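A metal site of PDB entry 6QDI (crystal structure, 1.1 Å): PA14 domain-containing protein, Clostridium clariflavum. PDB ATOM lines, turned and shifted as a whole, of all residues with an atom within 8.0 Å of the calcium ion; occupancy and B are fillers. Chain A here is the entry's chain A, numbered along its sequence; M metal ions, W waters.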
ATOM      1  N   PHE A   9       0.680  -0.740  16.755  1.00  0.00           N
ATOM      2  CA  PHE A   9       0.925  -2.060  16.198  1.00  0.00           C
ATOM      3  C   PHE A   9       0.102  -3.094  16.933  1.00  0.00           C
ATOM      4  O   PHE A   9      -0.076  -3.018  18.155  1.00  0.00           O
ATOM      5  CB  PHE A   9       2.415  -2.410  16.315  1.00  0.00           C
ATOM      6  CG  PHE A   9       3.300  -1.458  15.540  1.00  0.00           C
ATOM      7  CD1 PHE A   9       3.641  -1.741  14.219  1.00  0.00           C
ATOM      8  CD2 PHE A   9       3.835  -0.320  16.119  1.00  0.00           C
ATOM      9  CE1 PHE A   9       4.445  -0.869  13.505  1.00  0.00           C
ATOM     10  CE2 PHE A   9       4.644   0.545  15.386  1.00  0.00           C
ATOM     11  CZ  PHE A   9       4.944   0.243  14.094  1.00  0.00           C
ATOM     12  N   ASP A  10      -0.343  -4.097  16.208  1.00  0.00           N
ATOM     13  CA  ASP A  10      -1.252  -5.102  16.721  1.00  0.00           C
ATOM     14  C   ASP A  10      -0.551  -6.204  17.513  1.00  0.00           C
ATOM     15  O   ASP A  10      -1.233  -7.061  18.045  1.00  0.00           O
ATOM     16  CB  ASP A  10      -2.051  -5.775  15.577  1.00  0.00           C
ATOM     17  CG  ASP A  10      -3.579  -5.697  15.725  1.00  0.00           C
ATOM     18  OD1 ASP A  10      -4.098  -5.105  16.618  1.00  0.00           O
ATOM     19  OD2 ASP A  10      -4.298  -6.141  14.762  1.00  0.00           O
ATOM     20  N   ASN A  11       0.766  -6.214  17.555  1.00  0.00           N
ATOM     21  CA  ASN A  11       1.549  -7.230  18.272  1.00  0.00           C
ATOM     22  C   ASN A  11       2.386  -6.590  19.372  1.00  0.00           C
ATOM     23  O   ASN A  11       2.493  -5.356  19.443  1.00  0.00           O
ATOM     24  CB  ASN A  11       2.473  -7.948  17.264  1.00  0.00           C
ATOM     25  CG  ASN A  11       1.678  -8.703  16.239  1.00  0.00           C
ATOM     26  OD1 ASN A  11       0.667  -9.324  16.560  1.00  0.00           O
ATOM     27  ND2 ASN A  11       2.195  -8.746  15.022  1.00  0.00           N
ATOM     28  N   ILE A  12       3.036  -7.400  20.196  1.00  0.00           N
ATOM     29  CA  ILE A  12       3.885  -6.869  21.296  1.00  0.00           C
ATOM     30  C   ILE A  12       5.211  -6.296  20.828  1.00  0.00           C
ATOM     31  O   ILE A  12       5.889  -5.662  21.634  1.00  0.00           O
ATOM     32  CB  ILE A  12       4.186  -7.928  22.367  1.00  0.00           C
ATOM     33  CG1 ILE A  12       5.016  -9.103  21.844  1.00  0.00           C
ATOM     34  CG2 ILE A  12       2.875  -8.436  23.003  1.00  0.00           C
ATOM     35  CD1 ILE A  12       5.755  -9.833  22.938  1.00  0.00           C
ATOM     36  N   THR A  15       5.326  -4.843  15.330  1.00  0.00           N
ATOM     37  CA  THR A  15       4.980  -5.396  14.049  1.00  0.00           C
ATOM     38  C   THR A  15       3.455  -5.391  13.872  1.00  0.00           C
ATOM     39  O   THR A  15       2.695  -5.406  14.822  1.00  0.00           O
ATOM     40  CB  THR A  15       5.539  -6.790  13.827  1.00  0.00           C
ATOM     41  OG1 THR A  15       4.883  -7.732  14.664  1.00  0.00           O
ATOM     42  CG2 THR A  15       7.029  -6.832  13.963  1.00  0.00           C
ATOM     43  N   ASN A  16       3.076  -5.373  12.591  1.00  0.00           N
ATOM     44  CA  ASN A  16       1.682  -5.362  12.129  1.00  0.00           C
ATOM     45  C   ASN A  16       1.001  -4.040  12.453  1.00  0.00           C
ATOM     46  O   ASN A  16       0.149  -3.925  13.340  1.00  0.00           O
ATOM     47  CB  ASN A  16       0.889  -6.586  12.590  1.00  0.00           C
ATOM     48  CG  ASN A  16      -0.298  -6.797  11.739  1.00  0.00           C
ATOM     49  OD1 ASN A  16      -0.411  -6.216  10.644  1.00  0.00           O
ATOM     50  ND2 ASN A  16      -1.147  -7.697  12.153  1.00  0.00           N
ATOM     51  N   ILE A  39      -6.923  -1.527  16.708  1.00  0.00           N
ATOM     52  CA  ILE A  39      -6.050  -2.472  17.390  1.00  0.00           C
ATOM     53  C   ILE A  39      -6.928  -3.513  18.035  1.00  0.00           C
ATOM     54  O   ILE A  39      -7.806  -3.173  18.865  1.00  0.00           O
ATOM     55  CB  ILE A  39      -5.182  -1.725  18.438  1.00  0.00           C
ATOM     56  CG1 ILE A  39      -4.210  -0.760  17.748  1.00  0.00           C
ATOM     57  CG2 ILE A  39      -4.406  -2.679  19.328  1.00  0.00           C
ATOM     58  CD1 ILE A  39      -3.073  -1.451  17.000  1.00  0.00           C
ATOM     59  N   ARG A  40      -6.694  -4.784  17.700  1.00  0.00           N
ATOM     60  CA  ARG A  40      -7.473  -5.897  18.256  1.00  0.00           C
ATOM     61  C   ARG A  40      -7.432  -5.814  19.791  1.00  0.00           C
ATOM     62  O   ARG A  40      -6.363  -5.634  20.400  1.00  0.00           O
ATOM     63  CB  ARG A  40      -6.901  -7.257  17.772  1.00  0.00           C
ATOM     64  CG  ARG A  40      -7.721  -8.478  18.203  1.00  0.00           C
ATOM     65  CD  ARG A  40      -8.806  -8.782  17.161  1.00  0.00           C
ATOM     66  NE  ARG A  40      -8.035  -9.063  15.983  1.00  0.00           N
ATOM     67  CZ  ARG A  40      -7.678 -10.268  15.558  1.00  0.00           C
ATOM     68  NH1 ARG A  40      -8.091 -11.328  16.175  1.00  0.00           N
ATOM     69  NH2 ARG A  40      -6.863 -10.374  14.503  1.00  0.00           N
ATOM     70  N   ASN A  41      -8.574  -6.031  20.421  1.00  0.00           N
ATOM     71  CA  ASN A  41      -8.721  -5.912  21.879  1.00  0.00           C
ATOM     72  C   ASN A  41      -8.348  -7.230  22.548  1.00  0.00           C
ATOM     73  O   ASN A  41      -9.188  -7.886  23.161  1.00  0.00           O
ATOM     74  CB  ASN A  41     -10.147  -5.492  22.250  1.00  0.00           C
ATOM     75  CG  ASN A  41     -10.268  -5.157  23.680  1.00  0.00           C
ATOM     76  OD1 ASN A  41      -9.253  -4.818  24.325  1.00  0.00           O
ATOM     77  ND2 ASN A  41     -11.494  -5.167  24.188  1.00  0.00           N
ATOM     78  N   ASP A  42      -7.076  -7.599  22.425  1.00  0.00           N
ATOM     79  CA  ASP A  42      -6.585  -8.861  22.929  1.00  0.00           C
ATOM     80  C   ASP A  42      -5.486  -8.718  23.979  1.00  0.00           C
ATOM     81  O   ASP A  42      -4.908  -9.723  24.391  1.00  0.00           O
ATOM     82  CB  ASP A  42      -6.084  -9.759  21.803  1.00  0.00           C
ATOM     83  CG  ASP A  42      -4.866  -9.208  21.082  1.00  0.00           C
ATOM     84  OD1 ASP A  42      -4.414  -8.115  21.422  1.00  0.00           O
ATOM     85  OD2 ASP A  42      -4.332  -9.880  20.179  1.00  0.00           O
ATOM     86  N   GLU A  43      -5.150  -7.481  24.377  1.00  0.00           N
ATOM     87  CA  GLU A  43      -4.158  -7.220  25.419  1.00  0.00           C
ATOM     88  C   GLU A  43      -2.714  -7.377  24.978  1.00  0.00           C
ATOM     89  O   GLU A  43      -1.826  -7.361  25.816  1.00  0.00           O
ATOM     90  CB  GLU A  43      -4.434  -7.971  26.732  1.00  0.00           C
ATOM     91  CG  GLU A  43      -5.872  -7.950  27.191  1.00  0.00           C
ATOM     92  CD  GLU A  43      -6.127  -8.755  28.420  1.00  0.00           C
ATOM     93  OE1 GLU A  43      -5.159  -9.124  29.148  1.00  0.00           O
ATOM     94  OE2 GLU A  43      -7.332  -9.053  28.688  1.00  0.00           O
ATOM     95  N   SER A  44      -2.475  -7.494  23.655  1.00  0.00           N
ATOM     96  CA  SER A  44      -1.100  -7.582  23.126  1.00  0.00           C
ATOM     97  C   SER A  44      -0.904  -6.524  22.051  1.00  0.00           C
ATOM     98  O   SER A  44      -1.436  -6.663  20.950  1.00  0.00           O
ATOM     99  CB  SER A  44      -0.773  -8.955  22.611  1.00  0.00           C
ATOM    100  OG  SER A  44      -1.668  -9.400  21.632  1.00  0.00           O
ATOM    101  N   TYR A  45      -0.184  -5.448  22.341  1.00  0.00           N
ATOM    102  CA  TYR A  45      -0.036  -4.364  21.376  1.00  0.00           C
ATOM    103  C   TYR A  45       1.189  -3.562  21.721  1.00  0.00           C
ATOM    104  O   TYR A  45       1.806  -3.756  22.782  1.00  0.00           O
ATOM    105  CB  TYR A  45      -1.332  -3.484  21.304  1.00  0.00           C
ATOM    106  CG  TYR A  45      -1.753  -2.897  22.623  1.00  0.00           C
ATOM    107  CD1 TYR A  45      -1.185  -1.733  23.091  1.00  0.00           C
ATOM    108  CD2 TYR A  45      -2.720  -3.515  23.418  1.00  0.00           C
ATOM    109  CE1 TYR A  45      -1.563  -1.180  24.335  1.00  0.00           C
ATOM    110  CE2 TYR A  45      -3.099  -2.974  24.633  1.00  0.00           C
ATOM    111  CZ  TYR A  45      -2.503  -1.824  25.081  1.00  0.00           C
ATOM    112  OH  TYR A  45      -2.825  -1.267  26.306  1.00  0.00           O
ATOM    113  N   SER A  46       1.576  -2.676  20.819  1.00  0.00           N
ATOM    114  CA  SER A  46       2.774  -1.889  21.041  1.00  0.00           C
ATOM    115  C   SER A  46       2.647  -0.587  20.260  1.00  0.00           C
ATOM    116  O   SER A  46       1.790  -0.464  19.367  1.00  0.00           O
ATOM    117  CB  SER A  46       4.036  -2.687  20.676  1.00  0.00           C
ATOM    118  OG  SER A  46       3.994  -3.152  19.315  1.00  0.00           O
ATOM    119  N   ASN A 112       2.470  -3.538  25.567  1.00  0.00           N
ATOM    120  CA  ASN A 112       1.642  -4.232  26.550  1.00  0.00           C
ATOM    121  C   ASN A 112       1.631  -5.705  26.209  1.00  0.00           C
ATOM    122  O   ASN A 112       1.288  -6.076  25.092  1.00  0.00           O
ATOM    123  CB  ASN A 112       0.227  -3.707  26.620  1.00  0.00           C
ATOM    124  CG  ASN A 112      -0.515  -4.253  27.826  1.00  0.00           C
ATOM    125  OD1 ASN A 112       0.134  -4.673  28.781  1.00  0.00           O
ATOM    126  ND2 ASN A 112      -1.850  -4.269  27.810  1.00  0.00           N
ATOM    127  N   ASP A 180       0.307 -12.374  10.795  1.00  0.00           N
ATOM    128  CA  ASP A 180       1.513 -11.701  11.292  1.00  0.00           C
ATOM    129  C   ASP A 180       1.292 -11.408  12.753  1.00  0.00           C
ATOM    130  O   ASP A 180       0.921 -10.292  13.108  1.00  0.00           O
ATOM    131  CB  ASP A 180       1.732 -10.417  10.494  1.00  0.00           C
ATOM    132  CG  ASP A 180       3.016  -9.732  10.822  1.00  0.00           C
ATOM    133  OD1 ASP A 180       3.900 -10.367  11.392  1.00  0.00           O
ATOM    134  OD2 ASP A 180       3.166  -8.540  10.467  1.00  0.00           O
ATOM    135  N   PHE A 181       1.470 -12.417  13.595  1.00  0.00           N
ATOM    136  CA  PHE A 181       1.054 -12.353  14.987  1.00  0.00           C
ATOM    137  C   PHE A 181       2.208 -12.590  15.950  1.00  0.00           C
ATOM    138  O   PHE A 181       3.025 -13.495  15.775  1.00  0.00           O
ATOM    139  CB  PHE A 181       0.017 -13.445  15.287  1.00  0.00           C
ATOM    140  CG  PHE A 181      -1.337 -13.164  14.681  1.00  0.00           C
ATOM    141  CD1 PHE A 181      -2.189 -12.277  15.272  1.00  0.00           C
ATOM    142  CD2 PHE A 181      -1.724 -13.789  13.514  1.00  0.00           C
ATOM    143  CE1 PHE A 181      -3.429 -12.042  14.760  1.00  0.00           C
ATOM    144  CE2 PHE A 181      -2.951 -13.490  12.937  1.00  0.00           C
ATOM    145  CZ  PHE A 181      -3.814 -12.627  13.578  1.00  0.00           C
ATOM    146  N   ASN A 182       2.231 -11.796  17.030  1.00  0.00           N
ATOM    147  CA  ASN A 182       3.094 -12.045  18.169  1.00  0.00           C
ATOM    148  C   ASN A 182       2.335 -11.531  19.364  1.00  0.00           C
ATOM    149  O   ASN A 182       2.262 -10.321  19.602  1.00  0.00           O
ATOM    150  CB  ASN A 182       4.453 -11.401  18.004  1.00  0.00           C
ATOM    151  CG  ASN A 182       5.360 -11.686  19.190  1.00  0.00           C
ATOM    152  OD1 ASN A 182       4.922 -12.242  20.188  1.00  0.00           O
ATOM    153  ND2 ASN A 182       6.612 -11.284  19.085  1.00  0.00           N
ATOM    154  N   TRP A 183       1.696 -12.456  20.078  1.00  0.00           N
ATOM    155  CA  TRP A 183       0.822 -12.108  21.181  1.00  0.00           C
ATOM    156  C   TRP A 183       1.579 -12.040  22.515  1.00  0.00           C
ATOM    157  O   TRP A 183       0.939 -11.788  23.532  1.00  0.00           O
ATOM    158  CB  TRP A 183      -0.303 -13.139  21.334  1.00  0.00           C
ATOM    159  CG  TRP A 183      -1.181 -13.341  20.137  1.00  0.00           C
ATOM    160  CD1 TRP A 183      -2.252 -12.584  19.766  1.00  0.00           C
ATOM    161  CD2 TRP A 183      -1.098 -14.430  19.196  1.00  0.00           C
ATOM    162  NE1 TRP A 183      -2.810 -13.098  18.609  1.00  0.00           N
ATOM    163  CE2 TRP A 183      -2.148 -14.242  18.269  1.00  0.00           C
ATOM    164  CE3 TRP A 183      -0.278 -15.547  19.067  1.00  0.00           C
ATOM    165  CZ2 TRP A 183      -2.402 -15.171  17.229  1.00  0.00           C
ATOM    166  CZ3 TRP A 183      -0.494 -16.412  18.003  1.00  0.00           C
ATOM    167  CH2 TRP A 183      -1.543 -16.217  17.118  1.00  0.00           C
ATOM    168  N   GLY A 184       2.882 -12.315  22.542  1.00  0.00           N
ATOM    169  CA  GLY A 184       3.516 -12.560  23.835  1.00  0.00           C
ATOM    170  C   GLY A 184       2.825 -13.714  24.508  1.00  0.00           C
ATOM    171  O   GLY A 184       2.686 -14.784  23.905  1.00  0.00           O
ATOM    172  N   GLY A 186      -0.313 -13.404  25.563  1.00  0.00           N
ATOM    173  CA  GLY A 186      -1.740 -13.206  25.343  1.00  0.00           C
ATOM    174  C   GLY A 186      -2.354 -14.256  24.390  1.00  0.00           C
ATOM    175  O   GLY A 186      -1.653 -15.059  23.792  1.00  0.00           O
ATOM    176  N   SER A 187      -3.665 -14.167  24.298  1.00  0.00           N
ATOM    177  CA  SER A 187      -4.426 -15.030  23.389  1.00  0.00           C
ATOM    178  C   SER A 187      -4.910 -14.244  22.191  1.00  0.00           C
ATOM    179  O   SER A 187      -4.814 -13.017  22.150  1.00  0.00           O
ATOM    180  CB  SER A 187      -5.597 -15.653  24.150  1.00  0.00           C
ATOM    181  OG  SER A 187      -5.075 -16.464  25.169  1.00  0.00           O
ATOM    182  N   PRO A 188      -5.494 -14.934  21.179  1.00  0.00           N
ATOM    183  CA  PRO A 188      -5.849 -14.182  19.964  1.00  0.00           C
ATOM    184  C   PRO A 188      -7.073 -13.301  20.089  1.00  0.00           C
ATOM    185  O   PRO A 188      -7.299 -12.469  19.222  1.00  0.00           O
ATOM    186  CB  PRO A 188      -6.040 -15.321  18.920  1.00  0.00           C
ATOM    187  CG  PRO A 188      -5.165 -16.413  19.415  1.00  0.00           C
ATOM    188  CD  PRO A 188      -5.410 -16.378  20.909  1.00  0.00           C
ATOM    189  N   SER A 189      -7.856 -13.518  21.151  1.00  0.00           N
ATOM    190  CA  SER A 189      -9.060 -12.757  21.425  1.00  0.00           C
ATOM    191  C   SER A 189      -9.316 -12.921  22.902  1.00  0.00           C
ATOM    192  O   SER A 189      -8.907 -13.928  23.499  1.00  0.00           O
ATOM    193  CB  SER A 189     -10.253 -13.306  20.642  1.00  0.00           C
ATOM    194  OG  SER A 189     -11.416 -12.648  21.043  1.00  0.00           O
HETATM  195 CA    CA M   1      -2.628  -8.187  19.635  1.00  0.00          CA
HETATM  196  O   HOH W   1      -0.962  -9.783  18.785  1.00  0.00           O
HETATM  197  O   HOH W   2      -3.898  -6.227  19.194  1.00  0.00           O
HETATM  198  O   HOH W   3      -3.612  -8.892  17.459  1.00  0.00           O
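OD1 of Asp 10 is in hydrogen-bond range of N of Arg 40 (2.8 Å).
N of Asp 10 is in hydrogen-bond range of O of Asn 16.
The nearest printed residue that does not touch the calcium ion is Trp 183 (4.4 Å).
The calcium ion is bound by the backbone carbonyl oxygen (O) of Ser 44 (2.3 Å), water W2 (2.4 Å), the backbone carbonyl oxygen (O) of Asp 10 (2.4 Å), water W1 (2.5 Å), the side-chain carboxylate (OD2) of Asp 42 (2.5 Å), water W3 (2.5 Å), the side-chain hydroxyl (OG) of Ser 44 (2.5 Å) and the side-chain carboxylate (OD1) of Asp 42 (2.5 Å).
The calcium ion has eight donor atoms within binding distance.
Water W1 bridges the side-chain amide oxygen (OD1) of Asn 11 and the backbone carbonyl oxygen (O) of Asn 182.
Water W2 lies within hydrogen-bond range of the backbone carbonyl oxygen (O) of Arg 40 and the side-chain carboxylate (OD1) of Asp 10.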
